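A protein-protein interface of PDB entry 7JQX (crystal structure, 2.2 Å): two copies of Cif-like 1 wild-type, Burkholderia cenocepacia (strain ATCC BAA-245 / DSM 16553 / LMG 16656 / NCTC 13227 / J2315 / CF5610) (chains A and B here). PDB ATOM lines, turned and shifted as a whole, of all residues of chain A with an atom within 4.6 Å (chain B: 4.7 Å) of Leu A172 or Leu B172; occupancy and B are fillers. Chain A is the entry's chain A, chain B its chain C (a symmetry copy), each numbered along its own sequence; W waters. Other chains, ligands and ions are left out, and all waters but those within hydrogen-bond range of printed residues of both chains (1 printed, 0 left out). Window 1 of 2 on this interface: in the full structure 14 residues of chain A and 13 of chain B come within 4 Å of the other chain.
NE1 of Trp A168 is in hydrogen-bond range of OE1 of Gln B175 (3.3 Å). OE1 of Gln A175 lies within hydrogen-bond range of NE1 of Trp B168, 3.5 Å away.
The backbone carbonyl oxygen of Gly A171 lies within hydrogen-bond range of the side-chain amide nitrogen of Gln A175, 2.9 Å away. NE2 of His A173 lies within hydrogen-bond range of OH of Tyr A190 (2.8 Å). The backbone carbonyl oxygen of Gly B171 lies within hydrogen-bond range of the side-chain amide nitrogen of Gln B175 (3.0 Å).
Among the printed residues, merely in contact across the chains: Trp A168 with Gly B171, Trp A168 with Leu B172, Gly A171 with Trp B168, Leu A172 with Trp B168, Leu A172 with Leu B172, Leu A182 with Leu B182, Leu A182 with Ile B183, Ile A183 with Leu B182 and Tyr A190 with Leu B182.
Leu A172 touches just these residues of chain B: Trp B168 and Leu B172. Leu B172 touches two residues of chain A. Printed residues of chain A within 4 Å of Gln B175: Trp A168 (3.3 Å). Of the printed residues of chain A, Trp B168 touches Gly A171 (3.8 Å), Leu A172 (3.8 Å) and Gln A175 (3.4 Å). Of the printed residues of chain B, Leu A182 touches Leu B182 (3.5 Å) and Ile B183 (3.96 Å). Of the printed residues of chain B, Gly A171 touches Trp B168. Of the printed residues of chain A, Gly B171 touches Trp A168 (3.9 Å). The nearest residue of chain B that does not touch Leu A172 is Leu B182 (4.1 Å).
Hydrophobic or aromatic side chains of chain B that line the printed part of chain A: Trp B168, Leu B172, Leu B182 and Ile B183. Along chain B the printed residues that touch a printed residue of chain A span positions 168 to 183. Of the 12 printed residues of chain A, 7 touch a printed residue of chain B. Hydrophobic or aromatic side chains of chain A that line the printed part of chain B: Trp A168, Leu A172, Leu A182, Ile A183 and Tyr A190.
Trp A168 touches Gln B175, and with the chains exchanged Gln A175 touches Trp B168. Leu B172 touches its own counterpart, Leu A172. Leu A182 touches its own counterpart, Leu B182. Tyr A190 touches Leu B182, but with the chains exchanged Leu A182 does not touch Tyr B190 (4.1 Å). 12 positions are printed for both chains.
Water W1 lies within hydrogen-bond range of O of Trp B168, O of Trp A168, N of Leu A172 and N of Leu B172.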
ATOM      1  N   TRP A 168      19.836  -5.532 -29.206  1.00  0.00           N
ATOM      2  CA  TRP A 168      20.202  -6.946 -29.173  1.00  0.00           C
ATOM      3  C   TRP A 168      19.019  -7.848 -28.839  1.00  0.00           C
ATOM      4  O   TRP A 168      18.973  -8.999 -29.278  1.00  0.00           O
ATOM      5  CB  TRP A 168      21.321  -7.165 -28.152  1.00  0.00           C
ATOM      6  CG  TRP A 168      20.851  -7.010 -26.722  1.00  0.00           C
ATOM      7  CD1 TRP A 168      20.915  -5.881 -25.951  1.00  0.00           C
ATOM      8  CD2 TRP A 168      20.222  -8.013 -25.910  1.00  0.00           C
ATOM      9  NE1 TRP A 168      20.366  -6.124 -24.700  1.00  0.00           N
ATOM     10  CE2 TRP A 168      19.930  -7.424 -24.658  1.00  0.00           C
ATOM     11  CE3 TRP A 168      19.887  -9.355 -26.116  1.00  0.00           C
ATOM     12  CZ2 TRP A 168      19.322  -8.141 -23.619  1.00  0.00           C
ATOM     13  CZ3 TRP A 168      19.282 -10.051 -25.099  1.00  0.00           C
ATOM     14  CH2 TRP A 168      19.008  -9.452 -23.861  1.00  0.00           C
ATOM     15  N   HIS A 169      18.057  -7.355 -28.068  1.00  0.00           N
ATOM     16  CA  HIS A 169      16.990  -8.198 -27.541  1.00  0.00           C
ATOM     17  C   HIS A 169      15.885  -8.501 -28.550  1.00  0.00           C
ATOM     18  O   HIS A 169      15.031  -9.350 -28.263  1.00  0.00           O
ATOM     19  CB  HIS A 169      16.373  -7.523 -26.319  1.00  0.00           C
ATOM     20  CG  HIS A 169      15.875  -6.142 -26.594  1.00  0.00           C
ATOM     21  ND1 HIS A 169      16.722  -5.079 -26.821  1.00  0.00           N
ATOM     22  CD2 HIS A 169      14.616  -5.652 -26.712  1.00  0.00           C
ATOM     23  CE1 HIS A 169      16.006  -3.984 -27.035  1.00  0.00           C
ATOM     24  NE2 HIS A 169      14.725  -4.306 -26.979  1.00  0.00           N
ATOM     25  N   PHE A 170      15.858  -7.821 -29.699  1.00  0.00           N
ATOM     26  CA  PHE A 170      14.833  -8.106 -30.703  1.00  0.00           C
ATOM     27  C   PHE A 170      14.861  -9.578 -31.102  1.00  0.00           C
ATOM     28  O   PHE A 170      13.810 -10.215 -31.231  1.00  0.00           O
ATOM     29  CB  PHE A 170      15.039  -7.239 -31.949  1.00  0.00           C
ATOM     30  CG  PHE A 170      14.679  -5.790 -31.778  1.00  0.00           C
ATOM     31  CD1 PHE A 170      14.423  -5.254 -30.533  1.00  0.00           C
ATOM     32  CD2 PHE A 170      14.629  -4.955 -32.886  1.00  0.00           C
ATOM     33  CE1 PHE A 170      14.116  -3.906 -30.396  1.00  0.00           C
ATOM     34  CE2 PHE A 170      14.320  -3.624 -32.763  1.00  0.00           C
ATOM     35  CZ  PHE A 170      14.055  -3.091 -31.523  1.00  0.00           C
ATOM     36  N   GLY A 171      16.059 -10.125 -31.320  1.00  0.00           N
ATOM     37  CA  GLY A 171      16.204 -11.524 -31.663  1.00  0.00           C
ATOM     38  C   GLY A 171      15.599 -12.417 -30.593  1.00  0.00           C
ATOM     39  O   GLY A 171      14.656 -13.166 -30.870  1.00  0.00           O
ATOM     40  N   LEU A 172      16.078 -12.281 -29.351  1.00  0.00           N
ATOM     41  CA  LEU A 172      15.572 -13.111 -28.264  1.00  0.00           C
ATOM     42  C   LEU A 172      14.055 -13.008 -28.143  1.00  0.00           C
ATOM     43  O   LEU A 172      13.358 -14.028 -28.129  1.00  0.00           O
ATOM     44  CB  LEU A 172      16.243 -12.716 -26.942  1.00  0.00           C
ATOM     45  CG  LEU A 172      15.662 -13.348 -25.664  1.00  0.00           C
ATOM     46  CD1 LEU A 172      15.475 -14.887 -25.774  1.00  0.00           C
ATOM     47  CD2 LEU A 172      16.537 -13.000 -24.459  1.00  0.00           C
ATOM     48  N   HIS A 173      13.524 -11.779 -28.100  1.00  0.00           N
ATOM     49  CA  HIS A 173      12.087 -11.597 -27.894  1.00  0.00           C
ATOM     50  C   HIS A 173      11.276 -12.209 -29.022  1.00  0.00           C
ATOM     51  O   HIS A 173      10.125 -12.617 -28.809  1.00  0.00           O
ATOM     52  CB  HIS A 173      11.748 -10.109 -27.761  1.00  0.00           C
ATOM     53  CG  HIS A 173      12.266  -9.482 -26.504  1.00  0.00           C
ATOM     54  ND1 HIS A 173      11.848  -8.246 -26.057  1.00  0.00           N
ATOM     55  CD2 HIS A 173      13.157  -9.932 -25.591  1.00  0.00           C
ATOM     56  CE1 HIS A 173      12.469  -7.958 -24.928  1.00  0.00           C
ATOM     57  NE2 HIS A 173      13.270  -8.963 -24.624  1.00  0.00           N
ATOM     58  N   GLN A 174      11.858 -12.298 -30.217  1.00  0.00           N
ATOM     59  CA  GLN A 174      11.166 -12.867 -31.362  1.00  0.00           C
ATOM     60  C   GLN A 174      11.222 -14.389 -31.399  1.00  0.00           C
ATOM     61  O   GLN A 174      10.644 -14.982 -32.311  1.00  0.00           O
ATOM     62  CB  GLN A 174      11.721 -12.245 -32.654  1.00  0.00           C
ATOM     63  CG  GLN A 174      11.243 -10.805 -32.842  1.00  0.00           C
ATOM     64  CD  GLN A 174      11.880 -10.101 -34.016  1.00  0.00           C
ATOM     65  OE1 GLN A 174      12.948 -10.478 -34.483  1.00  0.00           O
ATOM     66  NE2 GLN A 174      11.235  -9.049 -34.484  1.00  0.00           N
ATOM     67  N   GLN A 175      11.882 -15.036 -30.434  1.00  0.00           N
ATOM     68  CA  GLN A 175      11.877 -16.503 -30.335  1.00  0.00           C
ATOM     69  C   GLN A 175      10.660 -16.941 -29.519  1.00  0.00           C
ATOM     70  O   GLN A 175      10.694 -16.923 -28.289  1.00  0.00           O
ATOM     71  CB  GLN A 175      13.167 -16.998 -29.691  1.00  0.00           C
ATOM     72  CG  GLN A 175      14.443 -16.549 -30.401  1.00  0.00           C
ATOM     73  CD  GLN A 175      14.310 -16.618 -31.903  1.00  0.00           C
ATOM     74  OE1 GLN A 175      14.159 -17.706 -32.478  1.00  0.00           O
ATOM     75  NE2 GLN A 175      14.333 -15.451 -32.551  1.00  0.00           N
ATOM     76  N   ALA A 179      11.818 -17.334 -25.466  1.00  0.00           N
ATOM     77  CA  ALA A 179      11.974 -16.136 -24.654  1.00  0.00           C
ATOM     78  C   ALA A 179      11.214 -16.285 -23.341  1.00  0.00           C
ATOM     79  O   ALA A 179      11.772 -16.047 -22.267  1.00  0.00           O
ATOM     80  CB  ALA A 179      11.497 -14.913 -25.439  1.00  0.00           C
ATOM     81  N   LEU A 182      12.935 -18.775 -20.914  1.00  0.00           N
ATOM     82  CA  LEU A 182      14.162 -18.303 -20.291  1.00  0.00           C
ATOM     83  C   LEU A 182      13.885 -17.261 -19.218  1.00  0.00           C
ATOM     84  O   LEU A 182      14.548 -17.249 -18.181  1.00  0.00           O
ATOM     85  CB  LEU A 182      15.084 -17.706 -21.341  1.00  0.00           C
ATOM     86  CG  LEU A 182      15.670 -18.681 -22.353  1.00  0.00           C
ATOM     87  CD1 LEU A 182      16.681 -17.940 -23.210  1.00  0.00           C
ATOM     88  CD2 LEU A 182      16.330 -19.833 -21.629  1.00  0.00           C
ATOM     89  N   ILE A 183      12.909 -16.387 -19.445  1.00  0.00           N
ATOM     90  CA  ILE A 183      12.732 -15.218 -18.596  1.00  0.00           C
ATOM     91  C   ILE A 183      11.650 -15.400 -17.523  1.00  0.00           C
ATOM     92  O   ILE A 183      11.655 -14.660 -16.524  1.00  0.00           O
ATOM     93  CB  ILE A 183      12.457 -13.985 -19.485  1.00  0.00           C
ATOM     94  CG1 ILE A 183      13.680 -13.727 -20.368  1.00  0.00           C
ATOM     95  CG2 ILE A 183      12.136 -12.720 -18.660  1.00  0.00           C
ATOM     96  CD1 ILE A 183      13.419 -12.846 -21.539  1.00  0.00           C
ATOM     97  N   TYR A 190      15.823  -9.510 -15.038  1.00  0.00           N
ATOM     98  CA  TYR A 190      15.951  -9.183 -16.452  1.00  0.00           C
ATOM     99  C   TYR A 190      15.553  -7.735 -16.724  1.00  0.00           C
ATOM    100  O   TYR A 190      16.267  -7.006 -17.425  1.00  0.00           O
ATOM    101  CB  TYR A 190      15.090 -10.134 -17.277  1.00  0.00           C
ATOM    102  CG  TYR A 190      15.204  -9.966 -18.773  1.00  0.00           C
ATOM    103  CD1 TYR A 190      16.299 -10.466 -19.472  1.00  0.00           C
ATOM    104  CD2 TYR A 190      14.207  -9.325 -19.489  1.00  0.00           C
ATOM    105  CE1 TYR A 190      16.389 -10.328 -20.857  1.00  0.00           C
ATOM    106  CE2 TYR A 190      14.286  -9.181 -20.850  1.00  0.00           C
ATOM    107  CZ  TYR A 190      15.381  -9.679 -21.533  1.00  0.00           C
ATOM    108  OH  TYR A 190      15.441  -9.531 -22.895  1.00  0.00           O
ATOM    109  N   TRP B 168      19.911 -14.986 -34.681  1.00  0.00           N
ATOM    110  CA  TRP B 168      19.231 -14.210 -33.653  1.00  0.00           C
ATOM    111  C   TRP B 168      19.951 -14.280 -32.311  1.00  0.00           C
ATOM    112  O   TRP B 168      19.909 -13.316 -31.529  1.00  0.00           O
ATOM    113  CB  TRP B 168      17.796 -14.714 -33.510  1.00  0.00           C
ATOM    114  CG  TRP B 168      17.722 -16.080 -32.879  1.00  0.00           C
ATOM    115  CD1 TRP B 168      17.635 -17.284 -33.520  1.00  0.00           C
ATOM    116  CD2 TRP B 168      17.720 -16.371 -31.477  1.00  0.00           C
ATOM    117  NE1 TRP B 168      17.579 -18.311 -32.597  1.00  0.00           N
ATOM    118  CE2 TRP B 168      17.633 -17.775 -31.338  1.00  0.00           C
ATOM    119  CE3 TRP B 168      17.774 -15.579 -30.325  1.00  0.00           C
ATOM    120  CZ2 TRP B 168      17.604 -18.399 -30.095  1.00  0.00           C
ATOM    121  CZ3 TRP B 168      17.748 -16.207 -29.087  1.00  0.00           C
ATOM    122  CH2 TRP B 168      17.668 -17.601 -28.987  1.00  0.00           C
ATOM    123  N   HIS B 169      20.633 -15.393 -32.034  1.00  0.00           N
ATOM    124  CA  HIS B 169      21.235 -15.634 -30.730  1.00  0.00           C
ATOM    125  C   HIS B 169      22.549 -14.900 -30.520  1.00  0.00           C
ATOM    126  O   HIS B 169      23.057 -14.907 -29.387  1.00  0.00           O
ATOM    127  CB  HIS B 169      21.476 -17.128 -30.533  1.00  0.00           C
ATOM    128  CG  HIS B 169      22.347 -17.737 -31.588  1.00  0.00           C
ATOM    129  ND1 HIS B 169      21.951 -17.845 -32.903  1.00  0.00           N
ATOM    130  CD2 HIS B 169      23.593 -18.263 -31.525  1.00  0.00           C
ATOM    131  CE1 HIS B 169      22.912 -18.422 -33.606  1.00  0.00           C
ATOM    132  NE2 HIS B 169      23.922 -18.679 -32.795  1.00  0.00           N
ATOM    133  N   PHE B 170      23.140 -14.305 -31.562  1.00  0.00           N
ATOM    134  CA  PHE B 170      24.394 -13.582 -31.343  1.00  0.00           C
ATOM    135  C   PHE B 170      24.207 -12.493 -30.290  1.00  0.00           C
ATOM    136  O   PHE B 170      25.011 -12.364 -29.356  1.00  0.00           O
ATOM    137  CB  PHE B 170      24.909 -12.961 -32.647  1.00  0.00           C
ATOM    138  CG  PHE B 170      25.533 -13.942 -33.621  1.00  0.00           C
ATOM    139  CD1 PHE B 170      25.395 -15.304 -33.462  1.00  0.00           C
ATOM    140  CD2 PHE B 170      26.256 -13.472 -34.711  1.00  0.00           C
ATOM    141  CE1 PHE B 170      25.949 -16.190 -34.371  1.00  0.00           C
ATOM    142  CE2 PHE B 170      26.818 -14.350 -35.621  1.00  0.00           C
ATOM    143  CZ  PHE B 170      26.668 -15.713 -35.446  1.00  0.00           C
ATOM    144  N   GLY B 171      23.127 -11.727 -30.405  1.00  0.00           N
ATOM    145  CA  GLY B 171      22.842 -10.677 -29.447  1.00  0.00           C
ATOM    146  C   GLY B 171      22.748 -11.194 -28.023  1.00  0.00           C
ATOM    147  O   GLY B 171      23.441 -10.689 -27.132  1.00  0.00           O
ATOM    148  N   LEU B 172      21.879 -12.184 -27.794  1.00  0.00           N
ATOM    149  CA  LEU B 172      21.723 -12.749 -26.455  1.00  0.00           C
ATOM    150  C   LEU B 172      23.050 -13.259 -25.913  1.00  0.00           C
ATOM    151  O   LEU B 172      23.411 -12.982 -24.762  1.00  0.00           O
ATOM    152  CB  LEU B 172      20.681 -13.866 -26.461  1.00  0.00           C
ATOM    153  CG  LEU B 172      20.609 -14.722 -25.182  1.00  0.00           C
ATOM    154  CD1 LEU B 172      20.305 -13.890 -23.932  1.00  0.00           C
ATOM    155  CD2 LEU B 172      19.564 -15.829 -25.348  1.00  0.00           C
ATOM    156  N   HIS B 173      23.787 -14.024 -26.729  1.00  0.00           N
ATOM    157  CA  HIS B 173      25.034 -14.624 -26.262  1.00  0.00           C
ATOM    158  C   HIS B 173      26.063 -13.559 -25.901  1.00  0.00           C
ATOM    159  O   HIS B 173      26.939 -13.791 -25.057  1.00  0.00           O
ATOM    160  CB  HIS B 173      25.577 -15.597 -27.320  1.00  0.00           C
ATOM    161  CG  HIS B 173      24.767 -16.851 -27.466  1.00  0.00           C
ATOM    162  ND1 HIS B 173      25.229 -17.966 -28.128  1.00  0.00           N
ATOM    163  CD2 HIS B 173      23.517 -17.161 -27.039  1.00  0.00           C
ATOM    164  CE1 HIS B 173      24.306 -18.914 -28.094  1.00  0.00           C
ATOM    165  NE2 HIS B 173      23.254 -18.449 -27.444  1.00  0.00           N
ATOM    166  N   GLN B 174      25.974 -12.392 -26.518  1.00  0.00           N
ATOM    167  CA  GLN B 174      26.894 -11.310 -26.188  1.00  0.00           C
ATOM    168  C   GLN B 174      26.488 -10.512 -24.943  1.00  0.00           C
ATOM    169  O   GLN B 174      27.239  -9.624 -24.533  1.00  0.00           O
ATOM    170  CB  GLN B 174      27.043 -10.388 -27.401  1.00  0.00           C
ATOM    171  CG  GLN B 174      27.893 -11.023 -28.491  1.00  0.00           C
ATOM    172  CD  GLN B 174      27.868 -10.275 -29.818  1.00  0.00           C
ATOM    173  OE1 GLN B 174      27.027  -9.421 -30.050  1.00  0.00           O
ATOM    174  NE2 GLN B 174      28.768 -10.644 -30.715  1.00  0.00           N
ATOM    175  N   GLN B 175      25.352 -10.809 -24.304  1.00  0.00           N
ATOM    176  CA  GLN B 175      24.987 -10.119 -23.062  1.00  0.00           C
ATOM    177  C   GLN B 175      25.623 -10.868 -21.892  1.00  0.00           C
ATOM    178  O   GLN B 175      25.071 -11.856 -21.404  1.00  0.00           O
ATOM    179  CB  GLN B 175      23.472 -10.031 -22.899  1.00  0.00           C
ATOM    180  CG  GLN B 175      22.734  -9.344 -24.059  1.00  0.00           C
ATOM    181  CD  GLN B 175      23.386  -8.056 -24.520  1.00  0.00           C
ATOM    182  OE1 GLN B 175      23.365  -7.032 -23.815  1.00  0.00           O
ATOM    183  NE2 GLN B 175      23.932  -8.084 -25.729  1.00  0.00           N
ATOM    184  N   ALA B 179      23.022 -13.726 -20.294  1.00  0.00           N
ATOM    185  CA  ALA B 179      22.818 -14.987 -21.006  1.00  0.00           C
ATOM    186  C   ALA B 179      22.967 -16.182 -20.064  1.00  0.00           C
ATOM    187  O   ALA B 179      22.129 -17.094 -20.055  1.00  0.00           O
ATOM    188  CB  ALA B 179      23.797 -15.078 -22.175  1.00  0.00           C
ATOM    189  N   LEU B 182      19.931 -16.525 -17.632  1.00  0.00           N
ATOM    190  CA  LEU B 182      18.679 -16.958 -18.244  1.00  0.00           C
ATOM    191  C   LEU B 182      18.703 -18.445 -18.584  1.00  0.00           C
ATOM    192  O   LEU B 182      17.673 -19.118 -18.472  1.00  0.00           O
ATOM    193  CB  LEU B 182      18.395 -16.124 -19.499  1.00  0.00           C
ATOM    194  CG  LEU B 182      18.003 -14.657 -19.290  1.00  0.00           C
ATOM    195  CD1 LEU B 182      17.583 -14.007 -20.607  1.00  0.00           C
ATOM    196  CD2 LEU B 182      16.903 -14.544 -18.242  1.00  0.00           C
ATOM    197  N   ILE B 183      19.860 -18.966 -19.019  1.00  0.00           N
ATOM    198  CA  ILE B 183      19.949 -20.312 -19.596  1.00  0.00           C
ATOM    199  C   ILE B 183      20.441 -21.364 -18.603  1.00  0.00           C
ATOM    200  O   ILE B 183      20.186 -22.565 -18.813  1.00  0.00           O
ATOM    201  CB  ILE B 183      20.851 -20.287 -20.850  1.00  0.00           C
ATOM    202  CG1 ILE B 183      20.249 -19.358 -21.906  1.00  0.00           C
ATOM    203  CG2 ILE B 183      21.053 -21.698 -21.461  1.00  0.00           C
ATOM    204  CD1 ILE B 183      21.198 -18.990 -23.025  1.00  0.00           C
ATOM    205  N   TYR B 190      17.194 -25.486 -23.986  1.00  0.00           N
ATOM    206  CA  TYR B 190      17.698 -24.441 -24.868  1.00  0.00           C
ATOM    207  C   TYR B 190      18.471 -25.044 -26.033  1.00  0.00           C
ATOM    208  O   TYR B 190      18.247 -24.685 -27.193  1.00  0.00           O
ATOM    209  CB  TYR B 190      18.605 -23.498 -24.085  1.00  0.00           C
ATOM    210  CG  TYR B 190      19.154 -22.321 -24.886  1.00  0.00           C
ATOM    211  CD1 TYR B 190      18.349 -21.231 -25.180  1.00  0.00           C
ATOM    212  CD2 TYR B 190      20.480 -22.292 -25.322  1.00  0.00           C
ATOM    213  CE1 TYR B 190      18.845 -20.140 -25.884  1.00  0.00           C
ATOM    214  CE2 TYR B 190      20.983 -21.204 -26.036  1.00  0.00           C
ATOM    215  CZ  TYR B 190      20.149 -20.130 -26.314  1.00  0.00           C
ATOM    216  OH  TYR B 190      20.586 -19.033 -27.023  1.00  0.00           O
HETATM  217  O   HOH W   1      19.098 -11.900 -29.156  1.00  0.00           O
